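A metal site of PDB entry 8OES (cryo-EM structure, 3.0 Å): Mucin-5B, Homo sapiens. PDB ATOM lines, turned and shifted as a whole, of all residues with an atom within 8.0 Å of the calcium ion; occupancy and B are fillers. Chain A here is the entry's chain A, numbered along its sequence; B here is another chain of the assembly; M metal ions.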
ATOM      1  N   THR A 880      -9.942  31.787   1.138  1.00  0.00           N
ATOM      2  CA  THR A 880     -10.438  32.080  -0.192  1.00  0.00           C
ATOM      3  C   THR A 880     -11.805  31.455  -0.404  1.00  0.00           C
ATOM      4  O   THR A 880     -12.404  30.864   0.490  1.00  0.00           O
ATOM      5  CB  THR A 880      -9.461  31.580  -1.244  1.00  0.00           C
ATOM      6  OG1 THR A 880     -10.191  31.349  -2.461  1.00  0.00           O
ATOM      7  CG2 THR A 880      -8.832  30.302  -0.810  1.00  0.00           C
ATOM      8  N   PHE A 881     -12.304  31.628  -1.630  1.00  0.00           N
ATOM      9  CA  PHE A 881     -13.645  31.176  -1.955  1.00  0.00           C
ATOM     10  C   PHE A 881     -13.764  29.660  -1.846  1.00  0.00           C
ATOM     11  O   PHE A 881     -14.770  29.147  -1.365  1.00  0.00           O
ATOM     12  CB  PHE A 881     -14.008  31.628  -3.372  1.00  0.00           C
ATOM     13  CG  PHE A 881     -14.473  33.055  -3.464  1.00  0.00           C
ATOM     14  CD1 PHE A 881     -15.671  33.453  -2.919  1.00  0.00           C
ATOM     15  CD2 PHE A 881     -13.709  33.988  -4.136  1.00  0.00           C
ATOM     16  CE1 PHE A 881     -16.087  34.757  -3.029  1.00  0.00           C
ATOM     17  CE2 PHE A 881     -14.125  35.292  -4.246  1.00  0.00           C
ATOM     18  CZ  PHE A 881     -15.311  35.673  -3.693  1.00  0.00           C
ATOM     19  N   ASP A 882     -12.743  28.939  -2.310  1.00  0.00           N
ATOM     20  CA  ASP A 882     -12.734  27.485  -2.333  1.00  0.00           C
ATOM     21  C   ASP A 882     -12.409  26.877  -0.973  1.00  0.00           C
ATOM     22  O   ASP A 882     -12.149  25.676  -0.912  1.00  0.00           O
ATOM     23  CB  ASP A 882     -11.723  26.970  -3.357  1.00  0.00           C
ATOM     24  CG  ASP A 882     -12.063  27.389  -4.757  1.00  0.00           C
ATOM     25  OD1 ASP A 882     -13.232  27.268  -5.151  1.00  0.00           O
ATOM     26  OD2 ASP A 882     -11.152  27.864  -5.457  1.00  0.00           O
ATOM     27  N   ASP A 884      -9.788  27.311   0.999  1.00  0.00           N
ATOM     28  CA  ASP A 884      -8.390  27.260   1.416  1.00  0.00           C
ATOM     29  C   ASP A 884      -8.085  28.385   2.394  1.00  0.00           C
ATOM     30  O   ASP A 884      -8.699  29.449   2.359  1.00  0.00           O
ATOM     31  CB  ASP A 884      -7.466  27.345   0.205  1.00  0.00           C
ATOM     32  CG  ASP A 884      -6.036  27.053   0.550  1.00  0.00           C
ATOM     33  OD1 ASP A 884      -5.758  26.707   1.714  1.00  0.00           O
ATOM     34  OD2 ASP A 884      -5.170  27.171  -0.337  1.00  0.00           O
ATOM     35  N   GLY A 995     -15.454  30.222 -11.095  1.00  0.00           N
ATOM     36  CA  GLY A 995     -14.395  29.866 -12.012  1.00  0.00           C
ATOM     37  C   GLY A 995     -13.830  31.000 -12.828  1.00  0.00           C
ATOM     38  O   GLY A 995     -12.827  30.796 -13.535  1.00  0.00           O
ATOM     39  N   CYS A1001      -8.455  35.817  -3.462  1.00  0.00           N
ATOM     40  CA  CYS A1001      -9.552  34.942  -3.056  1.00  0.00           C
ATOM     41  C   CYS A1001      -9.669  33.738  -3.984  1.00  0.00           C
ATOM     42  O   CYS A1001     -10.767  33.198  -4.161  1.00  0.00           O
ATOM     43  CB  CYS A1001     -10.872  35.708  -3.020  1.00  0.00           C
ATOM     44  SG  CYS A1001     -10.930  37.078  -1.847  1.00  0.00           S
ATOM     45  N   GLY A1002      -8.557  33.307  -4.566  1.00  0.00           N
ATOM     46  CA  GLY A1002      -8.575  32.154  -5.425  1.00  0.00           C
ATOM     47  C   GLY A1002      -9.349  32.444  -6.695  1.00  0.00           C
ATOM     48  O   GLY A1002      -9.661  33.581  -7.017  1.00  0.00           O
ATOM     49  N   ASN A1003      -9.649  31.365  -7.410  1.00  0.00           N
ATOM     50  CA  ASN A1003     -10.411  31.479  -8.649  1.00  0.00           C
ATOM     51  C   ASN A1003     -11.807  30.895  -8.537  1.00  0.00           C
ATOM     52  O   ASN A1003     -12.481  30.761  -9.552  1.00  0.00           O
ATOM     53  CB  ASN A1003      -9.640  30.819  -9.792  1.00  0.00           C
ATOM     54  CG  ASN A1003      -9.612  29.320  -9.688  1.00  0.00           C
ATOM     55  OD1 ASN A1003      -9.569  28.768  -8.595  1.00  0.00           O
ATOM     56  ND2 ASN A1003      -9.612  28.650 -10.823  1.00  0.00           N
ATOM     57  N   PHE A1004     -12.258  30.566  -7.325  1.00  0.00           N
ATOM     58  CA  PHE A1004     -13.621  30.129  -7.098  1.00  0.00           C
ATOM     59  C   PHE A1004     -14.006  28.996  -8.042  1.00  0.00           C
ATOM     60  O   PHE A1004     -14.898  29.124  -8.875  1.00  0.00           O
ATOM     61  CB  PHE A1004     -14.586  31.312  -7.244  1.00  0.00           C
ATOM     62  CG  PHE A1004     -15.962  31.052  -6.716  1.00  0.00           C
ATOM     63  CD1 PHE A1004     -16.234  29.953  -5.950  1.00  0.00           C
ATOM     64  CD2 PHE A1004     -16.984  31.949  -6.985  1.00  0.00           C
ATOM     65  CE1 PHE A1004     -17.509  29.741  -5.464  1.00  0.00           C
ATOM     66  CE2 PHE A1004     -18.253  31.729  -6.500  1.00  0.00           C
ATOM     67  CZ  PHE A1004     -18.512  30.628  -5.744  1.00  0.00           C
ATOM     68  N   ASP A1005     -13.296  27.882  -7.914  1.00  0.00           N
ATOM     69  CA  ASP A1005     -13.520  26.745  -8.794  1.00  0.00           C
ATOM     70  C   ASP A1005     -13.876  25.468  -8.044  1.00  0.00           C
ATOM     71  O   ASP A1005     -13.939  24.398  -8.656  1.00  0.00           O
ATOM     72  CB  ASP A1005     -12.295  26.502  -9.682  1.00  0.00           C
ATOM     73  CG  ASP A1005     -11.035  26.229  -8.880  1.00  0.00           C
ATOM     74  OD1 ASP A1005     -11.052  26.466  -7.655  1.00  0.00           O
ATOM     75  OD2 ASP A1005     -10.043  25.778  -9.469  1.00  0.00           O
ATOM     76  N   ASP A1006     -14.103  25.553  -6.729  1.00  0.00           N
ATOM     77  CA  ASP A1006     -14.285  24.377  -5.879  1.00  0.00           C
ATOM     78  C   ASP A1006     -13.116  23.406  -6.031  1.00  0.00           C
ATOM     79  O   ASP A1006     -13.288  22.196  -6.095  1.00  0.00           O
ATOM     80  CB  ASP A1006     -15.613  23.676  -6.187  1.00  0.00           C
ATOM     81  CG  ASP A1006     -16.755  24.641  -6.358  1.00  0.00           C
ATOM     82  OD1 ASP A1006     -16.649  25.523  -7.229  1.00  0.00           O
ATOM     83  OD2 ASP A1006     -17.751  24.518  -5.617  1.00  0.00           O
ATOM     84  N   ASN A1007     -11.915  23.973  -6.086  1.00  0.00           N
ATOM     85  CA  ASN A1007     -10.688  23.184  -6.179  1.00  0.00           C
ATOM     86  C   ASN A1007      -9.632  23.979  -5.426  1.00  0.00           C
ATOM     87  O   ASN A1007      -8.974  24.855  -5.997  1.00  0.00           O
ATOM     88  CB  ASN A1007     -10.282  22.927  -7.620  1.00  0.00           C
ATOM     89  CG  ASN A1007      -9.006  22.138  -7.745  1.00  0.00           C
ATOM     90  OD1 ASN A1007      -8.318  21.882  -6.761  1.00  0.00           O
ATOM     91  ND2 ASN A1007      -8.673  21.742  -8.970  1.00  0.00           N
ATOM     92  N   ALA A1008      -9.473  23.664  -4.145  1.00  0.00           N
ATOM     93  CA  ALA A1008      -8.677  24.501  -3.250  1.00  0.00           C
ATOM     94  C   ALA A1008      -7.185  24.225  -3.348  1.00  0.00           C
ATOM     95  O   ALA A1008      -6.398  25.022  -2.836  1.00  0.00           O
ATOM     96  CB  ALA A1008      -9.136  24.306  -1.811  1.00  0.00           C
ATOM     97  N   ILE A1009      -6.779  23.127  -3.979  1.00  0.00           N
ATOM     98  CA  ILE A1009      -5.363  22.820  -4.045  1.00  0.00           C
ATOM     99  C   ILE A1009      -4.642  23.779  -4.975  1.00  0.00           C
ATOM    100  O   ILE A1009      -3.516  24.208  -4.704  1.00  0.00           O
ATOM    101  CB  ILE A1009      -5.152  21.354  -4.467  1.00  0.00           C
ATOM    102  CG1 ILE A1009      -6.345  20.495  -4.026  1.00  0.00           C
ATOM    103  CG2 ILE A1009      -3.869  20.819  -3.859  1.00  0.00           C
ATOM    104  CD1 ILE A1009      -6.294  19.084  -4.550  1.00  0.00           C
ATOM    105  N   ASN A1010      -5.279  24.153  -6.086  1.00  0.00           N
ATOM    106  CA  ASN A1010      -4.669  24.992  -7.098  1.00  0.00           C
ATOM    107  C   ASN A1010      -4.998  26.469  -6.931  1.00  0.00           C
ATOM    108  O   ASN A1010      -4.685  27.264  -7.825  1.00  0.00           O
ATOM    109  CB  ASN A1010      -5.076  24.523  -8.499  1.00  0.00           C
ATOM    110  CG  ASN A1010      -6.295  25.230  -9.021  1.00  0.00           C
ATOM    111  OD1 ASN A1010      -7.308  25.342  -8.327  1.00  0.00           O
ATOM    112  ND2 ASN A1010      -6.200  25.740 -10.241  1.00  0.00           N
ATOM    113  N   ASP A1011      -5.618  26.858  -5.817  1.00  0.00           N
ATOM    114  CA  ASP A1011      -5.952  28.256  -5.615  1.00  0.00           C
ATOM    115  C   ASP A1011      -4.735  29.134  -5.445  1.00  0.00           C
ATOM    116  O   ASP A1011      -4.866  30.361  -5.468  1.00  0.00           O
ATOM    117  CB  ASP A1011      -6.868  28.422  -4.411  1.00  0.00           C
ATOM    118  CG  ASP A1011      -8.261  28.766  -4.795  1.00  0.00           C
ATOM    119  OD1 ASP A1011      -8.597  28.563  -5.985  1.00  0.00           O
ATOM    120  OD2 ASP A1011      -9.036  29.238  -3.942  1.00  0.00           O
ATOM    121  N   PHE A1012      -3.558  28.557  -5.256  1.00  0.00           N
ATOM    122  CA  PHE A1012      -2.329  29.347  -5.260  1.00  0.00           C
ATOM    123  C   PHE A1012      -1.858  29.560  -6.689  1.00  0.00           C
ATOM    124  O   PHE A1012      -0.710  29.271  -7.016  1.00  0.00           O
ATOM    125  CB  PHE A1012      -1.247  28.646  -4.453  1.00  0.00           C
ATOM    126  CG  PHE A1012      -1.322  28.898  -2.985  1.00  0.00           C
ATOM    127  CD1 PHE A1012      -2.509  29.262  -2.393  1.00  0.00           C
ATOM    128  CD2 PHE A1012      -0.198  28.787  -2.189  1.00  0.00           C
ATOM    129  CE1 PHE A1012      -2.580  29.490  -1.046  1.00  0.00           C
ATOM    130  CE2 PHE A1012      -0.253  29.026  -0.853  1.00  0.00           C
ATOM    131  CZ  PHE A1012      -1.449  29.386  -0.271  1.00  0.00           C
ATOM    132  N   ALA A1013      -2.738  30.075  -7.533  1.00  0.00           N
ATOM    133  CA  ALA A1013      -2.431  30.332  -8.934  1.00  0.00           C
ATOM    134  C   ALA A1013      -2.039  31.785  -9.106  1.00  0.00           C
ATOM    135  O   ALA A1013      -2.858  32.689  -8.891  1.00  0.00           O
ATOM    136  CB  ALA A1013      -3.628  29.985  -9.820  1.00  0.00           C
ATOM    137  N   VAL A1019       0.725  27.329 -10.602  1.00  0.00           N
ATOM    138  CA  VAL A1019       0.311  27.000  -9.230  1.00  0.00           C
ATOM    139  C   VAL A1019       1.534  26.675  -8.399  1.00  0.00           C
ATOM    140  O   VAL A1019       2.331  25.803  -8.742  1.00  0.00           O
ATOM    141  CB  VAL A1019      -0.684  25.837  -9.233  1.00  0.00           C
ATOM    142  CG1 VAL A1019      -0.769  25.224  -7.858  1.00  0.00           C
ATOM    143  CG2 VAL A1019      -2.052  26.337  -9.669  1.00  0.00           C
ATOM    144  N   GLN B 542     -10.898  16.492  -6.117  1.00  0.00           N
ATOM    145  CA  GLN B 542     -10.262  17.804  -6.204  1.00  0.00           C
ATOM    146  C   GLN B 542     -11.191  18.902  -5.705  1.00  0.00           C
ATOM    147  O   GLN B 542     -11.549  19.840  -6.406  1.00  0.00           O
ATOM    148  CB  GLN B 542      -9.781  18.073  -7.631  1.00  0.00           C
ATOM    149  CG  GLN B 542      -9.080  16.900  -8.276  1.00  0.00           C
ATOM    150  CD  GLN B 542      -8.079  16.245  -7.353  1.00  0.00           C
ATOM    151  OE1 GLN B 542      -7.384  16.912  -6.593  1.00  0.00           O
ATOM    152  NE2 GLN B 542      -7.975  14.935  -7.443  1.00  0.00           N
HETATM  153 CA    CA M   1      -8.910  26.711  -7.409  1.00  0.00          CA
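N of Asp 1005 lies within hydrogen-bond range of OD1 of Asp 882.
The side-chain amide oxygen of Asn 1007 lies close to the backbone NH of Ile 1009, 3.4 Å away.
OD1 of Asp 1011 sits close to OD2 of Asp 882, 2.7 Å away.
OG1 of Thr 880 is in hydrogen-bond range of OD2 of Asp 1011 (2.8 Å).
The backbone carbonyl oxygen (O) of Asn 1003 lies close to the backbone NH (N) of Gly 995.
The side-chain carboxylate (OD2) of Asp 882 lies within hydrogen-bond range of the backbone NH (N) of Phe 1004 (3.5 Å).
The side-chain carboxylate (OD1) of Asp 882 lies within hydrogen-bond range of the backbone NH (N) of Asp 1006 (2.5 Å).
OD2 of Asp 882 touches the calcium ion (3.2 Å).
Within 4 Å of the calcium ion: Asp 882, Asn 1003, Asp 1005, Asn 1007, Asn 1010 and Asp 1011.
The nearest printed residue that does not touch the calcium ion is Ala 1008 (4.5 Å).
The side-chain carboxylate (OD1) of Asp 1005 binds the calcium ion (2.2 Å).
OD1 of Asn 1010 is bound to the calcium ion (2.3 Å).
O of Asn 1007 is bound to the calcium ion (2.3 Å).
The side-chain carboxylate (OD1) of Asp 1011 is bound to the calcium ion.
The side-chain amide oxygen (OD1) of Asn 1003 binds the calcium ion (2.5 Å).
The side-chain carboxylate (OD2) of Asp 1005 is bound to the calcium ion, at 2.5 Å.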
